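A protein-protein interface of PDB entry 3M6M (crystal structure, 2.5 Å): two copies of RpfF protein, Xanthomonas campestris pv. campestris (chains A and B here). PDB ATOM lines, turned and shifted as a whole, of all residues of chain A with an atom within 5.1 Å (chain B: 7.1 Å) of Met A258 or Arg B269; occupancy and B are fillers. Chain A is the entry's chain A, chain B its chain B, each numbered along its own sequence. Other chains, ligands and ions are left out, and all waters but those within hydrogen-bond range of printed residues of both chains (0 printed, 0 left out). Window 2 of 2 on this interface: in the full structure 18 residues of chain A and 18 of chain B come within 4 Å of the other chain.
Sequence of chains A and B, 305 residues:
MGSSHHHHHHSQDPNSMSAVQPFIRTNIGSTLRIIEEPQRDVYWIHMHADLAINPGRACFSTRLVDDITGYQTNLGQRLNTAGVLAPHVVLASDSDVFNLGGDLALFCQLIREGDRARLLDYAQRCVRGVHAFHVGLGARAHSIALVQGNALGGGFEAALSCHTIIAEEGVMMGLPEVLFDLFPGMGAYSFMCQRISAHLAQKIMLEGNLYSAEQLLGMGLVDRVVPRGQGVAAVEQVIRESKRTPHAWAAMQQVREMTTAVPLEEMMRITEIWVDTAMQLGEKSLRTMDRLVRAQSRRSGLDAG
NH2 of Arg B269 is in salt-bridge range of OE1 of Glu B265, at 2.9 Å.
The backbone carbonyl oxygen (O) of Val A255 lies within hydrogen-bond range of the side-chain hydroxyl (OG1) of Thr A259 (2.6 Å).
The indole nitrogen (NE1) of Trp B274 is in hydrogen-bond range of the backbone carbonyl oxygen (O) of Phe B183 (2.9 Å).
Met A258 touches just these residues of chain B: Glu B266, Arg B269, Ile B270 and Ile B273.
Of the printed residues of chain A, Arg B269 touches Met A258 (3.6 Å).
Of the printed residues of chain A, Phe B183 touches Val A255.
Of the printed residues of chain A, Glu B266 touches Met A258 and Thr A259.
Of the printed residues of chain A, Ile B273 touches Gln A254 and Met A258.
Printed residues of chain B within 4 Å of Val A255: Phe B183 (3.8 Å).
Of the printed residues of chain B, Gln A254 touches Ile B273 (3.5 Å).
Thr B271 touches none of the printed residues of chain A.
The nearest residue of chain B that does not touch Met A258 is Glu B265 (5.3 Å).
The nearest printed residue of chain A that does not touch Phe B183 is Gln A254 (7.0 Å).
Of the 7 printed residues of chain A, 4 touch a printed residue of chain B.
Hydrophobic or aromatic side chains of chain A within 4 Å of the printed part of chain B: Val A255 and Met A258.
Printed residues of chain B that touch a printed residue of chain A: Phe B183, Glu B266, Arg B269, Ile B270 and Ile B273.
Hydrophobic or aromatic side chains of chain B that line the printed part of chain A: Phe B183, Ile B270 and Ile B273.
Among the printed residues, no Asp or Glu carboxylate lies within 4 Å of a Lys or Arg side-chain nitrogen of the other chain.
Gln A254 touches Ile B273.
CG2 of Val A255 touches CE1 of Phe B183, at 3.8 Å.
Met A258 touches Glu B266.
CE of Met A258 touches CB of Arg B269, at 3.6 Å.
CE of Met A258 touches CG1 of Ile B270, at 3.8 Å.
Met A258 touches Ile B273 (SD to CD1, 3.7 Å).
Thr A259 touches Glu B266 (CG2 to OE2, 3.9 Å).
No position is printed for both chains.
Of the 7 pairs that touch across the chains among the printed residues, none has its exchanged pair printed and touching as well.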
ATOM      1  N   GLN A 254      12.002   6.061  35.439  1.00  0.00           N
ATOM      2  CA  GLN A 254      11.973   6.367  34.007  1.00  0.00           C
ATOM      3  C   GLN A 254      10.558   6.223  33.452  1.00  0.00           C
ATOM      4  O   GLN A 254      10.128   7.031  32.625  1.00  0.00           O
ATOM      5  CB  GLN A 254      12.921   5.454  33.225  1.00  0.00           C
ATOM      6  CG  GLN A 254      14.395   5.600  33.566  1.00  0.00           C
ATOM      7  CD  GLN A 254      15.273   4.636  32.779  1.00  0.00           C
ATOM      8  OE1 GLN A 254      15.338   4.696  31.552  1.00  0.00           O
ATOM      9  NE2 GLN A 254      15.952   3.743  33.489  1.00  0.00           N
ATOM     10  N   VAL A 255       9.844   5.197  33.918  1.00  0.00           N
ATOM     11  CA  VAL A 255       8.466   4.942  33.496  1.00  0.00           C
ATOM     12  C   VAL A 255       7.542   6.052  34.001  1.00  0.00           C
ATOM     13  O   VAL A 255       6.667   6.519  33.268  1.00  0.00           O
ATOM     14  CB  VAL A 255       7.972   3.542  33.958  1.00  0.00           C
ATOM     15  CG1 VAL A 255       6.478   3.358  33.678  1.00  0.00           C
ATOM     16  CG2 VAL A 255       8.774   2.444  33.273  1.00  0.00           C
ATOM     17  N   ARG A 256       7.757   6.475  35.245  1.00  0.00           N
ATOM     18  CA  ARG A 256       7.041   7.616  35.813  1.00  0.00           C
ATOM     19  C   ARG A 256       7.288   8.889  35.006  1.00  0.00           C
ATOM     20  O   ARG A 256       6.338   9.588  34.648  1.00  0.00           O
ATOM     21  CB  ARG A 256       7.440   7.842  37.269  1.00  0.00           C
ATOM     22  CG  ARG A 256       6.827   6.858  38.251  1.00  0.00           C
ATOM     23  CD  ARG A 256       7.445   7.010  39.635  1.00  0.00           C
ATOM     24  NE  ARG A 256       6.888   8.145  40.372  1.00  0.00           N
ATOM     25  CZ  ARG A 256       7.488   9.325  40.527  1.00  0.00           C
ATOM     26  NH1 ARG A 256       8.687   9.556  40.005  1.00  0.00           N
ATOM     27  NH2 ARG A 256       6.885  10.281  41.217  1.00  0.00           N
ATOM     28  N   GLU A 257       8.561   9.169  34.713  1.00  0.00           N
ATOM     29  CA  GLU A 257       8.975  10.346  33.938  1.00  0.00           C
ATOM     30  C   GLU A 257       8.174  10.516  32.643  1.00  0.00           C
ATOM     31  O   GLU A 257       7.772  11.628  32.305  1.00  0.00           O
ATOM     32  CB  GLU A 257      10.479  10.296  33.614  1.00  0.00           C
ATOM     33  CG  GLU A 257      11.424  10.546  34.799  1.00  0.00           C
ATOM     34  CD  GLU A 257      12.899  10.250  34.476  1.00  0.00           C
ATOM     35  OE1 GLU A 257      13.292  10.349  33.288  1.00  0.00           O
ATOM     36  OE2 GLU A 257      13.668   9.925  35.412  1.00  0.00           O
ATOM     37  N   MET A 258       7.941   9.410  31.936  1.00  0.00           N
ATOM     38  CA  MET A 258       7.253   9.438  30.642  1.00  0.00           C
ATOM     39  C   MET A 258       5.737   9.201  30.719  1.00  0.00           C
ATOM     40  O   MET A 258       5.064   9.185  29.688  1.00  0.00           O
ATOM     41  CB  MET A 258       7.903   8.451  29.660  1.00  0.00           C
ATOM     42  CG  MET A 258       7.873   6.997  30.109  1.00  0.00           C
ATOM     43  SD  MET A 258       7.921   5.853  28.735  1.00  0.00           S
ATOM     44  CE  MET A 258       6.271   6.053  28.060  1.00  0.00           C
ATOM     45  N   THR A 259       5.201   9.015  31.924  1.00  0.00           N
ATOM     46  CA  THR A 259       3.758   8.776  32.083  1.00  0.00           C
ATOM     47  C   THR A 259       3.087   9.713  33.091  1.00  0.00           C
ATOM     48  O   THR A 259       2.576  10.767  32.715  1.00  0.00           O
ATOM     49  CB  THR A 259       3.425   7.297  32.451  1.00  0.00           C
ATOM     50  OG1 THR A 259       4.117   6.925  33.649  1.00  0.00           O
ATOM     51  CG2 THR A 259       3.798   6.341  31.320  1.00  0.00           C
ATOM     52  N   THR A 260       3.105   9.329  34.366  1.00  0.00           N
ATOM     53  CA  THR A 260       2.283   9.973  35.396  1.00  0.00           C
ATOM     54  C   THR A 260       2.979  11.058  36.211  1.00  0.00           C
ATOM     55  O   THR A 260       2.324  11.737  37.006  1.00  0.00           O
ATOM     56  CB  THR A 260       1.708   8.938  36.388  1.00  0.00           C
ATOM     57  OG1 THR A 260       2.776   8.144  36.917  1.00  0.00           O
ATOM     58  CG2 THR A 260       0.685   8.034  35.697  1.00  0.00           C
ATOM     59  N   VAL B 127       4.389  -6.462  23.469  1.00  0.00           N
ATOM     60  CA  VAL B 127       3.566  -5.258  23.572  1.00  0.00           C
ATOM     61  C   VAL B 127       2.419  -5.272  22.556  1.00  0.00           C
ATOM     62  O   VAL B 127       1.272  -4.993  22.911  1.00  0.00           O
ATOM     63  CB  VAL B 127       4.427  -3.970  23.436  1.00  0.00           C
ATOM     64  CG1 VAL B 127       3.573  -2.753  23.100  1.00  0.00           C
ATOM     65  CG2 VAL B 127       5.209  -3.727  24.713  1.00  0.00           C
ATOM     66  N   PHE B 183      11.388  -5.151  36.149  1.00  0.00           N
ATOM     67  CA  PHE B 183      10.025  -4.678  36.376  1.00  0.00           C
ATOM     68  C   PHE B 183       9.102  -5.165  35.251  1.00  0.00           C
ATOM     69  O   PHE B 183       9.582  -5.509  34.169  1.00  0.00           O
ATOM     70  CB  PHE B 183       9.990  -3.147  36.501  1.00  0.00           C
ATOM     71  CG  PHE B 183      10.077  -2.422  35.184  1.00  0.00           C
ATOM     72  CD1 PHE B 183       8.922  -1.974  34.546  1.00  0.00           C
ATOM     73  CD2 PHE B 183      11.309  -2.186  34.583  1.00  0.00           C
ATOM     74  CE1 PHE B 183       8.989  -1.301  33.327  1.00  0.00           C
ATOM     75  CE2 PHE B 183      11.392  -1.512  33.365  1.00  0.00           C
ATOM     76  CZ  PHE B 183      10.229  -1.068  32.732  1.00  0.00           C
ATOM     77  N   LEU B 264      -0.360   2.739  22.020  1.00  0.00           N
ATOM     78  CA  LEU B 264       0.697   1.780  21.685  1.00  0.00           C
ATOM     79  C   LEU B 264       2.095   2.366  21.897  1.00  0.00           C
ATOM     80  O   LEU B 264       2.960   1.716  22.488  1.00  0.00           O
ATOM     81  CB  LEU B 264       0.536   1.291  20.236  1.00  0.00           C
ATOM     82  CG  LEU B 264       1.493   0.216  19.698  1.00  0.00           C
ATOM     83  CD1 LEU B 264       1.325  -1.112  20.439  1.00  0.00           C
ATOM     84  CD2 LEU B 264       1.293   0.018  18.204  1.00  0.00           C
ATOM     85  N   GLU B 265       2.289   3.597  21.420  1.00  0.00           N
ATOM     86  CA  GLU B 265       3.559   4.320  21.521  1.00  0.00           C
ATOM     87  C   GLU B 265       4.077   4.422  22.960  1.00  0.00           C
ATOM     88  O   GLU B 265       5.272   4.238  23.207  1.00  0.00           O
ATOM     89  CB  GLU B 265       3.419   5.712  20.880  1.00  0.00           C
ATOM     90  CG  GLU B 265       4.650   6.621  20.982  1.00  0.00           C
ATOM     91  CD  GLU B 265       4.500   7.738  22.017  1.00  0.00           C
ATOM     92  OE1 GLU B 265       4.002   7.484  23.140  1.00  0.00           O
ATOM     93  OE2 GLU B 265       4.891   8.885  21.701  1.00  0.00           O
ATOM     94  N   GLU B 266       3.171   4.708  23.894  1.00  0.00           N
ATOM     95  CA  GLU B 266       3.499   4.793  25.315  1.00  0.00           C
ATOM     96  C   GLU B 266       4.080   3.469  25.822  1.00  0.00           C
ATOM     97  O   GLU B 266       5.098   3.457  26.516  1.00  0.00           O
ATOM     98  CB  GLU B 266       2.258   5.194  26.122  1.00  0.00           C
ATOM     99  CG  GLU B 266       2.500   5.451  27.607  1.00  0.00           C
ATOM    100  CD  GLU B 266       1.264   5.980  28.320  1.00  0.00           C
ATOM    101  OE1 GLU B 266       0.815   7.098  27.989  1.00  0.00           O
ATOM    102  OE2 GLU B 266       0.747   5.283  29.217  1.00  0.00           O
ATOM    103  N   MET B 267       3.435   2.365  25.455  1.00  0.00           N
ATOM    104  CA  MET B 267       3.884   1.029  25.853  1.00  0.00           C
ATOM    105  C   MET B 267       5.221   0.652  25.211  1.00  0.00           C
ATOM    106  O   MET B 267       6.055   0.000  25.844  1.00  0.00           O
ATOM    107  CB  MET B 267       2.818  -0.018  25.526  1.00  0.00           C
ATOM    108  CG  MET B 267       1.581   0.066  26.414  1.00  0.00           C
ATOM    109  SD  MET B 267       0.343  -1.213  26.098  1.00  0.00           S
ATOM    110  CE  MET B 267       1.177  -2.648  26.764  1.00  0.00           C
ATOM    111  N   MET B 268       5.418   1.075  23.963  1.00  0.00           N
ATOM    112  CA  MET B 268       6.672   0.838  23.245  1.00  0.00           C
ATOM    113  C   MET B 268       7.857   1.522  23.920  1.00  0.00           C
ATOM    114  O   MET B 268       8.943   0.944  24.014  1.00  0.00           O
ATOM    115  CB  MET B 268       6.561   1.290  21.784  1.00  0.00           C
ATOM    116  CG  MET B 268       5.750   0.353  20.902  1.00  0.00           C
ATOM    117  SD  MET B 268       6.470  -1.302  20.766  1.00  0.00           S
ATOM    118  CE  MET B 268       5.279  -2.091  19.692  1.00  0.00           C
ATOM    119  N   ARG B 269       7.634   2.747  24.392  1.00  0.00           N
ATOM    120  CA  ARG B 269       8.662   3.502  25.109  1.00  0.00           C
ATOM    121  C   ARG B 269       8.956   2.917  26.493  1.00  0.00           C
ATOM    122  O   ARG B 269      10.071   3.046  26.996  1.00  0.00           O
ATOM    123  CB  ARG B 269       8.280   4.979  25.209  1.00  0.00           C
ATOM    124  CG  ARG B 269       8.452   5.759  23.908  1.00  0.00           C
ATOM    125  CD  ARG B 269       8.292   7.258  24.126  1.00  0.00           C
ATOM    126  NE  ARG B 269       6.937   7.638  24.471  1.00  0.00           N
ATOM    127  CZ  ARG B 269       6.545   8.617  25.286  1.00  0.00           C
ATOM    128  NH1 ARG B 269       7.395   9.405  25.945  1.00  0.00           N
ATOM    129  NH2 ARG B 269       5.241   8.784  25.442  1.00  0.00           N
ATOM    130  N   ILE B 270       7.960   2.267  27.093  1.00  0.00           N
ATOM    131  CA  ILE B 270       8.137   1.587  28.378  1.00  0.00           C
ATOM    132  C   ILE B 270       9.010   0.332  28.235  1.00  0.00           C
ATOM    133  O   ILE B 270       9.846   0.059  29.101  1.00  0.00           O
ATOM    134  CB  ILE B 270       6.773   1.283  29.072  1.00  0.00           C
ATOM    135  CG1 ILE B 270       6.114   2.592  29.526  1.00  0.00           C
ATOM    136  CG2 ILE B 270       6.952   0.354  30.273  1.00  0.00           C
ATOM    137  CD1 ILE B 270       4.641   2.470  29.904  1.00  0.00           C
ATOM    138  N   THR B 271       8.832  -0.414  27.140  1.00  0.00           N
ATOM    139  CA  THR B 271       9.686  -1.581  26.867  1.00  0.00           C
ATOM    140  C   THR B 271      11.110  -1.217  26.466  1.00  0.00           C
ATOM    141  O   THR B 271      12.027  -2.016  26.654  1.00  0.00           O
ATOM    142  CB  THR B 271       9.094  -2.552  25.819  1.00  0.00           C
ATOM    143  OG1 THR B 271       8.335  -1.827  24.845  1.00  0.00           O
ATOM    144  CG2 THR B 271       8.215  -3.582  26.491  1.00  0.00           C
ATOM    145  N   GLU B 272      11.289  -0.020  25.909  1.00  0.00           N
ATOM    146  CA  GLU B 272      12.619   0.535  25.660  1.00  0.00           C
ATOM    147  C   GLU B 272      13.397   0.669  26.972  1.00  0.00           C
ATOM    148  O   GLU B 272      14.580   0.333  27.043  1.00  0.00           O
ATOM    149  CB  GLU B 272      12.513   1.903  24.982  1.00  0.00           C
ATOM    150  CG  GLU B 272      12.299   1.853  23.471  1.00  0.00           C
ATOM    151  CD  GLU B 272      13.595   1.955  22.679  1.00  0.00           C
ATOM    152  OE1 GLU B 272      14.685   1.973  23.290  1.00  0.00           O
ATOM    153  OE2 GLU B 272      13.518   2.019  21.434  1.00  0.00           O
ATOM    154  N   ILE B 273      12.717   1.163  28.002  1.00  0.00           N
ATOM    155  CA  ILE B 273      13.298   1.293  29.335  1.00  0.00           C
ATOM    156  C   ILE B 273      13.533  -0.093  29.930  1.00  0.00           C
ATOM    157  O   ILE B 273      14.568  -0.343  30.556  1.00  0.00           O
ATOM    158  CB  ILE B 273      12.396   2.154  30.250  1.00  0.00           C
ATOM    159  CG1 ILE B 273      12.336   3.591  29.715  1.00  0.00           C
ATOM    160  CG2 ILE B 273      12.893   2.127  31.700  1.00  0.00           C
ATOM    161  CD1 ILE B 273      11.070   4.340  30.074  1.00  0.00           C
ATOM    162  N   TRP B 274      12.573  -0.987  29.699  1.00  0.00           N
ATOM    163  CA  TRP B 274      12.644  -2.373  30.155  1.00  0.00           C
ATOM    164  C   TRP B 274      13.874  -3.102  29.612  1.00  0.00           C
ATOM    165  O   TRP B 274      14.600  -3.739  30.377  1.00  0.00           O
ATOM    166  CB  TRP B 274      11.361  -3.117  29.777  1.00  0.00           C
ATOM    167  CG  TRP B 274      11.269  -4.516  30.310  1.00  0.00           C
ATOM    168  CD1 TRP B 274      10.782  -4.897  31.522  1.00  0.00           C
ATOM    169  CD2 TRP B 274      11.662  -5.720  29.638  1.00  0.00           C
ATOM    170  NE1 TRP B 274      10.850  -6.264  31.654  1.00  0.00           N
ATOM    171  CE2 TRP B 274      11.388  -6.793  30.512  1.00  0.00           C
ATOM    172  CE3 TRP B 274      12.223  -5.994  28.384  1.00  0.00           C
ATOM    173  CZ2 TRP B 274      11.654  -8.125  30.170  1.00  0.00           C
ATOM    174  CZ3 TRP B 274      12.489  -7.316  28.047  1.00  0.00           C
ATOM    175  CH2 TRP B 274      12.206  -8.364  28.938  1.00  0.00           C
